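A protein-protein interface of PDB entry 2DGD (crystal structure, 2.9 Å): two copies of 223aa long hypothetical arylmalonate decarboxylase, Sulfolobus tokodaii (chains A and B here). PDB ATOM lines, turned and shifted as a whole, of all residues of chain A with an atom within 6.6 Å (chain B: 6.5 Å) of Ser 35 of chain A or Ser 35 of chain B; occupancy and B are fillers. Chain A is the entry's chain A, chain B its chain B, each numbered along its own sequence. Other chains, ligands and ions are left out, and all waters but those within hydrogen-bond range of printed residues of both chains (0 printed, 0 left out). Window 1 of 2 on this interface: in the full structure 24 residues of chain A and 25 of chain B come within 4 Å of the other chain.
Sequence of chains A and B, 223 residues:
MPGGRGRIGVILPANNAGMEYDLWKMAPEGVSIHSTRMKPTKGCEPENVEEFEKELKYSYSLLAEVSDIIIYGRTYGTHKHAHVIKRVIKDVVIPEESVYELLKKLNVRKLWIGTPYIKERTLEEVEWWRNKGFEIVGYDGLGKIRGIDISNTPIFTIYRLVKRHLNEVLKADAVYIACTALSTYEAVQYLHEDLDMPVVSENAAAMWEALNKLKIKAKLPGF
Printed residues of chain B that touch a printed residue of chain A: Glu 20, Ile 33, His 34, Ser 35, Thr 36, Arg 37 and Leu 63. Hydrophobic or aromatic side chains of chain A that line the printed part of chain B: His 34 and Leu 63. Among the printed residues, no Asp or Glu carboxylate lies within 4 Å of a Lys or Arg side-chain nitrogen of the other chain.
The backbone carbonyl oxygen of Val 10 of chain A sits at hydrogen-bond distance from the backbone NH of Thr 36 of chain A, 3.2 Å away. The backbone carbonyl oxygen (O) of Thr 36 of chain A sits at hydrogen-bond distance from the backbone NH (N) of Leu 12 of chain A (3.2 Å). OE2 of Glu 20 of chain A sits at hydrogen-bond distance from OG of Ser 35 of chain A (2.7 Å). The backbone carbonyl oxygen of His 34 of chain B is in hydrogen-bond range of the backbone NH of Val 10 of chain B (2.7 Å). The backbone NH (N) of Leu 12 of chain B is in hydrogen-bond range of the backbone carbonyl oxygen (O) of Thr 36 of chain B, 3.2 Å away. The side-chain hydroxyl (OG) of Ser 35 of chain B lies within hydrogen-bond range of the side-chain carboxylate (OE2) of Glu 20 of chain B (2.6 Å).
Among the printed residues, pairs that only touch across the chains: Leu 63 of chain A with Arg 37 of chain B (3.2 Å), Arg 37 of chain A with Leu 63 of chain B (3.3 Å), His 34 of chain A with Arg 37 of chain B (3.6 Å), Arg 37 of chain A with His 34 of chain B (3.7 Å), Ile 33 of chain A with Glu 20 of chain B (3.8 Å), Thr 36 of chain A with Thr 36 of chain B (3.8 Å) and Glu 20 of chain A with Ile 33 of chain B (3.97 Å).
Of the printed residues of chain B, Ser 35 of chain A touches Glu 20, Ser 35 and Arg 37. Ser 35 of chain B touches three residues of chain A. Of the printed residues of chain A, Arg 37 of chain B touches His 34 (3.6 Å), Ser 35 (2.8 Å), Thr 36 (3.2 Å) and Leu 63 (3.2 Å). Of the printed residues of chain A, Ile 33 of chain B touches Glu 20 (3.97 Å). The nearest printed residue of chain B that does not touch Ser 35 of chain A is Thr 36 of chain B (4.01 Å). The nearest printed residue of chain A that does not touch His 34 of chain B is Ser 35 of chain A (5.4 Å).
Glu 20 of chain A touches Ile 33 of chain B, and with the chains exchanged Ile 33 of chain A touches Glu 20 of chain B. Glu 20 of chain A touches His 34 of chain B, and with the chains exchanged His 34 of chain A touches Glu 20 of chain B. His 34 of chain A touches Arg 37 of chain B, and with the chains exchanged Arg 37 of chain A touches His 34 of chain B. Ser 35 of chain A touches Arg 37 of chain B, and with the chains exchanged Arg 37 of chain A touches Ser 35 of chain B. Positions printed for both chains: 8, 9, 10, 11, 12, 20, 33, 34, 35, 36, 37 and 63. Of the 16 pairs that touch across the chains among the printed residues, 16 have their exchanged pair printed and touching as well.
The side-chain carboxylate (OE1) of Glu 20 of chain A is in hydrogen-bond range of a ring nitrogen (ND1) of His 34 of chain B (2.7 Å). OE2 of Glu 20 of chain A lies within hydrogen-bond range of N of Ser 35 of chain B (3.3 Å). The side-chain carboxylate of Glu 20 of chain B sits at hydrogen-bond distance from a ring nitrogen (ND1) of His 34 of chain A (2.6 Å). The backbone NH (N) of Ser 35 of chain A lies within hydrogen-bond range of the side-chain carboxylate (OE2) of Glu 20 of chain B (3.3 Å). The side-chain hydroxyl of Ser 35 of chain A sits at hydrogen-bond distance from the side-chain hydroxyl of Ser 35 of chain B (3.2 Å). O of Ser 35 of chain A lies within hydrogen-bond range of NH2 of Arg 37 of chain B (2.8 Å). The side-chain hydroxyl (OG1) of Thr 36 of chain A sits at hydrogen-bond distance from the backbone NH (N) of Arg 37 of chain B. NH2 of Arg 37 of chain A lies within hydrogen-bond range of O of Ser 35 of chain B (2.8 Å). The side-chain hydroxyl (OG1) of Thr 36 of chain B is in hydrogen-bond range of the backbone NH (N) of Arg 37 of chain A (3.2 Å).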
ATOM      1  N   ILE A   8     -13.940  22.476   3.973  1.00  0.00           N
ATOM      2  CA  ILE A   8     -13.112  23.657   3.790  1.00  0.00           C
ATOM      3  C   ILE A   8     -13.774  24.682   2.879  1.00  0.00           C
ATOM      4  O   ILE A   8     -14.089  24.404   1.720  1.00  0.00           O
ATOM      5  CB  ILE A   8     -11.736  23.274   3.197  1.00  0.00           C
ATOM      6  CG1 ILE A   8     -11.040  22.272   4.123  1.00  0.00           C
ATOM      7  CG2 ILE A   8     -10.870  24.515   3.022  1.00  0.00           C
ATOM      8  CD1 ILE A   8      -9.726  21.757   3.596  1.00  0.00           C
ATOM      9  N   GLY A   9     -13.994  25.873   3.418  1.00  0.00           N
ATOM     10  CA  GLY A   9     -14.599  26.928   2.633  1.00  0.00           C
ATOM     11  C   GLY A   9     -13.499  27.729   1.966  1.00  0.00           C
ATOM     12  O   GLY A   9     -12.403  27.855   2.508  1.00  0.00           O
ATOM     13  N   VAL A  10     -13.772  28.261   0.784  1.00  0.00           N
ATOM     14  CA  VAL A  10     -12.773  29.053   0.092  1.00  0.00           C
ATOM     15  C   VAL A  10     -13.393  30.262  -0.618  1.00  0.00           C
ATOM     16  O   VAL A  10     -14.370  30.138  -1.366  1.00  0.00           O
ATOM     17  CB  VAL A  10     -11.981  28.180  -0.926  1.00  0.00           C
ATOM     18  CG1 VAL A  10     -12.925  27.559  -1.925  1.00  0.00           C
ATOM     19  CG2 VAL A  10     -10.941  29.020  -1.645  1.00  0.00           C
ATOM     20  N   ILE A  11     -12.838  31.437  -0.349  1.00  0.00           N
ATOM     21  CA  ILE A  11     -13.298  32.657  -0.987  1.00  0.00           C
ATOM     22  C   ILE A  11     -12.295  32.947  -2.093  1.00  0.00           C
ATOM     23  O   ILE A  11     -11.103  33.082  -1.828  1.00  0.00           O
ATOM     24  CB  ILE A  11     -13.307  33.848  -0.010  1.00  0.00           C
ATOM     25  CG1 ILE A  11     -14.256  33.568   1.151  1.00  0.00           C
ATOM     26  CG2 ILE A  11     -13.729  35.115  -0.746  1.00  0.00           C
ATOM     27  CD1 ILE A  11     -14.187  34.610   2.232  1.00  0.00           C
ATOM     28  N   LEU A  12     -12.758  33.035  -3.333  1.00  0.00           N
ATOM     29  CA  LEU A  12     -11.834  33.303  -4.425  1.00  0.00           C
ATOM     30  C   LEU A  12     -12.349  34.284  -5.459  1.00  0.00           C
ATOM     31  O   LEU A  12     -13.541  34.560  -5.525  1.00  0.00           O
ATOM     32  CB  LEU A  12     -11.428  31.990  -5.111  1.00  0.00           C
ATOM     33  CG  LEU A  12     -12.474  30.878  -5.229  1.00  0.00           C
ATOM     34  CD1 LEU A  12     -13.661  31.366  -6.007  1.00  0.00           C
ATOM     35  CD2 LEU A  12     -11.862  29.675  -5.907  1.00  0.00           C
ATOM     36  N   GLU A  20     -10.063  25.789  -7.304  1.00  0.00           N
ATOM     37  CA  GLU A  20     -11.072  24.821  -6.905  1.00  0.00           C
ATOM     38  C   GLU A  20     -10.657  23.421  -7.324  1.00  0.00           C
ATOM     39  O   GLU A  20     -10.826  22.462  -6.575  1.00  0.00           O
ATOM     40  CB  GLU A  20     -12.422  25.206  -7.509  1.00  0.00           C
ATOM     41  CG  GLU A  20     -12.974  26.489  -6.908  1.00  0.00           C
ATOM     42  CD  GLU A  20     -14.086  27.096  -7.724  1.00  0.00           C
ATOM     43  OE1 GLU A  20     -13.860  27.362  -8.918  1.00  0.00           O
ATOM     44  OE2 GLU A  20     -15.186  27.319  -7.177  1.00  0.00           O
ATOM     45  N   TRP A  24      -9.783  20.293  -4.615  1.00  0.00           N
ATOM     46  CA  TRP A  24     -10.495  19.020  -4.612  1.00  0.00           C
ATOM     47  C   TRP A  24      -9.554  17.846  -4.843  1.00  0.00           C
ATOM     48  O   TRP A  24      -9.691  16.798  -4.223  1.00  0.00           O
ATOM     49  CB  TRP A  24     -11.597  19.007  -5.674  1.00  0.00           C
ATOM     50  CG  TRP A  24     -12.903  19.569  -5.182  1.00  0.00           C
ATOM     51  CD1 TRP A  24     -13.393  20.834  -5.384  1.00  0.00           C
ATOM     52  CD2 TRP A  24     -13.872  18.889  -4.374  1.00  0.00           C
ATOM     53  NE1 TRP A  24     -14.605  20.978  -4.754  1.00  0.00           N
ATOM     54  CE2 TRP A  24     -14.925  19.803  -4.126  1.00  0.00           C
ATOM     55  CE3 TRP A  24     -13.953  17.597  -3.833  1.00  0.00           C
ATOM     56  CZ2 TRP A  24     -16.048  19.463  -3.361  1.00  0.00           C
ATOM     57  CZ3 TRP A  24     -15.069  17.262  -3.072  1.00  0.00           C
ATOM     58  CH2 TRP A  24     -16.102  18.193  -2.845  1.00  0.00           C
ATOM     59  N   ILE A  33     -14.878  20.678  -0.441  1.00  0.00           N
ATOM     60  CA  ILE A  33     -14.538  22.081  -0.637  1.00  0.00           C
ATOM     61  C   ILE A  33     -15.783  22.883  -1.014  1.00  0.00           C
ATOM     62  O   ILE A  33     -16.562  22.474  -1.876  1.00  0.00           O
ATOM     63  CB  ILE A  33     -13.485  22.220  -1.760  1.00  0.00           C
ATOM     64  CG1 ILE A  33     -12.321  21.263  -1.497  1.00  0.00           C
ATOM     65  CG2 ILE A  33     -12.980  23.651  -1.835  1.00  0.00           C
ATOM     66  CD1 ILE A  33     -11.616  21.496  -0.168  1.00  0.00           C
ATOM     67  N   HIS A  34     -15.965  24.031  -0.370  1.00  0.00           N
ATOM     68  CA  HIS A  34     -17.124  24.880  -0.638  1.00  0.00           C
ATOM     69  C   HIS A  34     -16.651  26.294  -0.906  1.00  0.00           C
ATOM     70  O   HIS A  34     -15.984  26.898  -0.065  1.00  0.00           O
ATOM     71  CB  HIS A  34     -18.055  24.832   0.561  1.00  0.00           C
ATOM     72  CG  HIS A  34     -18.378  23.437   0.983  1.00  0.00           C
ATOM     73  ND1 HIS A  34     -19.240  22.629   0.273  1.00  0.00           N
ATOM     74  CD2 HIS A  34     -17.875  22.669   1.980  1.00  0.00           C
ATOM     75  CE1 HIS A  34     -19.253  21.424   0.812  1.00  0.00           C
ATOM     76  NE2 HIS A  34     -18.433  21.420   1.849  1.00  0.00           N
ATOM     77  N   SER A  35     -17.000  26.826  -2.071  1.00  0.00           N
ATOM     78  CA  SER A  35     -16.545  28.160  -2.421  1.00  0.00           C
ATOM     79  C   SER A  35     -17.614  29.192  -2.750  1.00  0.00           C
ATOM     80  O   SER A  35     -18.780  28.872  -2.978  1.00  0.00           O
ATOM     81  CB  SER A  35     -15.565  28.064  -3.593  1.00  0.00           C
ATOM     82  OG  SER A  35     -16.136  27.345  -4.672  1.00  0.00           O
ATOM     83  N   THR A  36     -17.182  30.445  -2.754  1.00  0.00           N
ATOM     84  CA  THR A  36     -18.035  31.568  -3.095  1.00  0.00           C
ATOM     85  C   THR A  36     -17.089  32.596  -3.705  1.00  0.00           C
ATOM     86  O   THR A  36     -15.937  32.710  -3.289  1.00  0.00           O
ATOM     87  CB  THR A  36     -18.755  32.151  -1.866  1.00  0.00           C
ATOM     88  OG1 THR A  36     -19.785  33.034  -2.316  1.00  0.00           O
ATOM     89  CG2 THR A  36     -17.781  32.921  -0.971  1.00  0.00           C
ATOM     90  N   ARG A  37     -17.570  33.334  -4.699  1.00  0.00           N
ATOM     91  CA  ARG A  37     -16.727  34.307  -5.383  1.00  0.00           C
ATOM     92  C   ARG A  37     -16.904  35.762  -4.989  1.00  0.00           C
ATOM     93  O   ARG A  37     -17.916  36.153  -4.403  1.00  0.00           O
ATOM     94  CB  ARG A  37     -16.924  34.172  -6.892  1.00  0.00           C
ATOM     95  CG  ARG A  37     -16.438  32.854  -7.434  1.00  0.00           C
ATOM     96  CD  ARG A  37     -16.754  32.691  -8.901  1.00  0.00           C
ATOM     97  NE  ARG A  37     -15.716  31.914  -9.562  1.00  0.00           N
ATOM     98  CZ  ARG A  37     -15.400  30.664  -9.250  1.00  0.00           C
ATOM     99  NH1 ARG A  37     -14.429  30.053  -9.907  1.00  0.00           N
ATOM    100  NH2 ARG A  37     -16.061  30.023  -8.297  1.00  0.00           N
ATOM    101  N   LEU A  63     -20.258  31.438   3.773  1.00  0.00           N
ATOM    102  CA  LEU A  63     -19.470  30.224   3.980  1.00  0.00           C
ATOM    103  C   LEU A  63     -19.351  29.794   5.445  1.00  0.00           C
ATOM    104  O   LEU A  63     -19.020  28.639   5.739  1.00  0.00           O
ATOM    105  CB  LEU A  63     -18.065  30.440   3.412  1.00  0.00           C
ATOM    106  CG  LEU A  63     -17.605  29.764   2.117  1.00  0.00           C
ATOM    107  CD1 LEU A  63     -18.753  29.501   1.193  1.00  0.00           C
ATOM    108  CD2 LEU A  63     -16.578  30.656   1.447  1.00  0.00           C
ATOM    109  N   ILE B   8     -18.287  23.742 -15.538  1.00  0.00           N
ATOM    110  CA  ILE B   8     -19.666  23.944 -15.140  1.00  0.00           C
ATOM    111  C   ILE B   8     -19.766  24.850 -13.927  1.00  0.00           C
ATOM    112  O   ILE B   8     -19.217  24.550 -12.867  1.00  0.00           O
ATOM    113  CB  ILE B   8     -20.342  22.594 -14.817  1.00  0.00           C
ATOM    114  CG1 ILE B   8     -20.255  21.676 -16.041  1.00  0.00           C
ATOM    115  CG2 ILE B   8     -21.795  22.817 -14.399  1.00  0.00           C
ATOM    116  CD1 ILE B   8     -20.828  20.295 -15.812  1.00  0.00           C
ATOM    117  N   GLY B   9     -20.466  25.965 -14.091  1.00  0.00           N
ATOM    118  CA  GLY B   9     -20.644  26.889 -12.989  1.00  0.00           C
ATOM    119  C   GLY B   9     -21.915  26.539 -12.246  1.00  0.00           C
ATOM    120  O   GLY B   9     -22.879  26.062 -12.842  1.00  0.00           O
ATOM    121  N   VAL B  10     -21.931  26.760 -10.942  1.00  0.00           N
ATOM    122  CA  VAL B  10     -23.122  26.452 -10.174  1.00  0.00           C
ATOM    123  C   VAL B  10     -23.413  27.516  -9.111  1.00  0.00           C
ATOM    124  O   VAL B  10     -22.531  27.898  -8.327  1.00  0.00           O
ATOM    125  CB  VAL B  10     -23.005  25.037  -9.506  1.00  0.00           C
ATOM    126  CG1 VAL B  10     -21.794  24.972  -8.629  1.00  0.00           C
ATOM    127  CG2 VAL B  10     -24.242  24.723  -8.697  1.00  0.00           C
ATOM    128  N   ILE B  11     -24.650  28.011  -9.110  1.00  0.00           N
ATOM    129  CA  ILE B  11     -25.073  28.999  -8.123  1.00  0.00           C
ATOM    130  C   ILE B  11     -25.886  28.238  -7.084  1.00  0.00           C
ATOM    131  O   ILE B  11     -26.891  27.613  -7.421  1.00  0.00           O
ATOM    132  CB  ILE B  11     -25.972  30.080  -8.740  1.00  0.00           C
ATOM    133  CG1 ILE B  11     -25.208  30.849  -9.817  1.00  0.00           C
ATOM    134  CG2 ILE B  11     -26.446  31.025  -7.659  1.00  0.00           C
ATOM    135  CD1 ILE B  11     -26.084  31.810 -10.591  1.00  0.00           C
ATOM    136  N   LEU B  12     -25.460  28.276  -5.825  1.00  0.00           N
ATOM    137  CA  LEU B  12     -26.191  27.543  -4.801  1.00  0.00           C
ATOM    138  C   LEU B  12     -26.353  28.295  -3.500  1.00  0.00           C
ATOM    139  O   LEU B  12     -25.667  29.281  -3.256  1.00  0.00           O
ATOM    140  CB  LEU B  12     -25.517  26.188  -4.535  1.00  0.00           C
ATOM    141  CG  LEU B  12     -23.988  26.093  -4.616  1.00  0.00           C
ATOM    142  CD1 LEU B  12     -23.356  27.029  -3.619  1.00  0.00           C
ATOM    143  CD2 LEU B  12     -23.552  24.674  -4.342  1.00  0.00           C
ATOM    144  N   GLU B  20     -22.103  20.393  -4.260  1.00  0.00           N
ATOM    145  CA  GLU B  20     -20.751  20.531  -4.794  1.00  0.00           C
ATOM    146  C   GLU B  20     -20.060  19.164  -4.807  1.00  0.00           C
ATOM    147  O   GLU B  20     -19.377  18.805  -5.772  1.00  0.00           O
ATOM    148  CB  GLU B  20     -19.956  21.545  -3.965  1.00  0.00           C
ATOM    149  CG  GLU B  20     -20.466  22.966  -4.154  1.00  0.00           C
ATOM    150  CD  GLU B  20     -19.979  23.928  -3.090  1.00  0.00           C
ATOM    151  OE1 GLU B  20     -20.202  23.656  -1.894  1.00  0.00           O
ATOM    152  OE2 GLU B  20     -19.384  24.964  -3.450  1.00  0.00           O
ATOM    153  N   ILE B  33     -15.893  21.953 -11.685  1.00  0.00           N
ATOM    154  CA  ILE B  33     -17.066  22.636 -11.163  1.00  0.00           C
ATOM    155  C   ILE B  33     -16.652  23.923 -10.458  1.00  0.00           C
ATOM    156  O   ILE B  33     -15.707  23.929  -9.672  1.00  0.00           O
ATOM    157  CB  ILE B  33     -17.801  21.721 -10.170  1.00  0.00           C
ATOM    158  CG1 ILE B  33     -18.032  20.347 -10.807  1.00  0.00           C
ATOM    159  CG2 ILE B  33     -19.128  22.341  -9.759  1.00  0.00           C
ATOM    160  CD1 ILE B  33     -18.856  20.374 -12.079  1.00  0.00           C
ATOM    161  N   HIS B  34     -17.364  25.012 -10.742  1.00  0.00           N
ATOM    162  CA  HIS B  34     -17.063  26.321 -10.147  1.00  0.00           C
ATOM    163  C   HIS B  34     -18.339  26.907  -9.564  1.00  0.00           C
ATOM    164  O   HIS B  34     -19.339  27.075 -10.265  1.00  0.00           O
ATOM    165  CB  HIS B  34     -16.480  27.233 -11.217  1.00  0.00           C
ATOM    166  CG  HIS B  34     -15.353  26.600 -11.965  1.00  0.00           C
ATOM    167  ND1 HIS B  34     -14.098  26.446 -11.420  1.00  0.00           N
ATOM    168  CD2 HIS B  34     -15.323  25.967 -13.161  1.00  0.00           C
ATOM    169  CE1 HIS B  34     -13.345  25.740 -12.243  1.00  0.00           C
ATOM    170  NE2 HIS B  34     -14.065  25.434 -13.306  1.00  0.00           N
ATOM    171  N   SER B  35     -18.301  27.223  -8.276  1.00  0.00           N
ATOM    172  CA  SER B  35     -19.492  27.729  -7.621  1.00  0.00           C
ATOM    173  C   SER B  35     -19.370  29.055  -6.906  1.00  0.00           C
ATOM    174  O   SER B  35     -18.281  29.538  -6.616  1.00  0.00           O
ATOM    175  CB  SER B  35     -20.012  26.684  -6.624  1.00  0.00           C
ATOM    176  OG  SER B  35     -19.006  26.304  -5.702  1.00  0.00           O
ATOM    177  N   THR B  36     -20.527  29.636  -6.635  1.00  0.00           N
ATOM    178  CA  THR B  36     -20.624  30.889  -5.914  1.00  0.00           C
ATOM    179  C   THR B  36     -21.944  30.791  -5.149  1.00  0.00           C
ATOM    180  O   THR B  36     -22.912  30.193  -5.632  1.00  0.00           O
ATOM    181  CB  THR B  36     -20.630  32.110  -6.857  1.00  0.00           C
ATOM    182  OG1 THR B  36     -20.419  33.302  -6.090  1.00  0.00           O
ATOM    183  CG2 THR B  36     -21.955  32.223  -7.592  1.00  0.00           C
ATOM    184  N   ARG B  37     -21.979  31.364  -3.952  1.00  0.00           N
ATOM    185  CA  ARG B  37     -23.168  31.290  -3.115  1.00  0.00           C
ATOM    186  C   ARG B  37     -24.058  32.516  -3.082  1.00  0.00           C
ATOM    187  O   ARG B  37     -23.651  33.617  -3.444  1.00  0.00           O
ATOM    188  CB  ARG B  37     -22.761  30.929  -1.688  1.00  0.00           C
ATOM    189  CG  ARG B  37     -22.170  29.540  -1.578  1.00  0.00           C
ATOM    190  CD  ARG B  37     -21.665  29.245  -0.187  1.00  0.00           C
ATOM    191  NE  ARG B  37     -21.822  27.833   0.132  1.00  0.00           N
ATOM    192  CZ  ARG B  37     -21.251  26.843  -0.539  1.00  0.00           C
ATOM    193  NH1 ARG B  37     -21.470  25.593  -0.170  1.00  0.00           N
ATOM    194  NH2 ARG B  37     -20.452  27.103  -1.565  1.00  0.00           N
ATOM    195  N   LEU B  63     -19.664  34.112 -12.305  1.00  0.00           N
ATOM    196  CA  LEU B  63     -19.442  32.801 -12.907  1.00  0.00           C
ATOM    197  C   LEU B  63     -19.399  32.814 -14.436  1.00  0.00           C
ATOM    198  O   LEU B  63     -18.912  31.874 -15.060  1.00  0.00           O
ATOM    199  CB  LEU B  63     -20.558  31.853 -12.445  1.00  0.00           C
ATOM    200  CG  LEU B  63     -20.311  30.730 -11.432  1.00  0.00           C
ATOM    201  CD1 LEU B  63     -19.190  31.068 -10.493  1.00  0.00           C
ATOM    202  CD2 LEU B  63     -21.591  30.488 -10.669  1.00  0.00           C
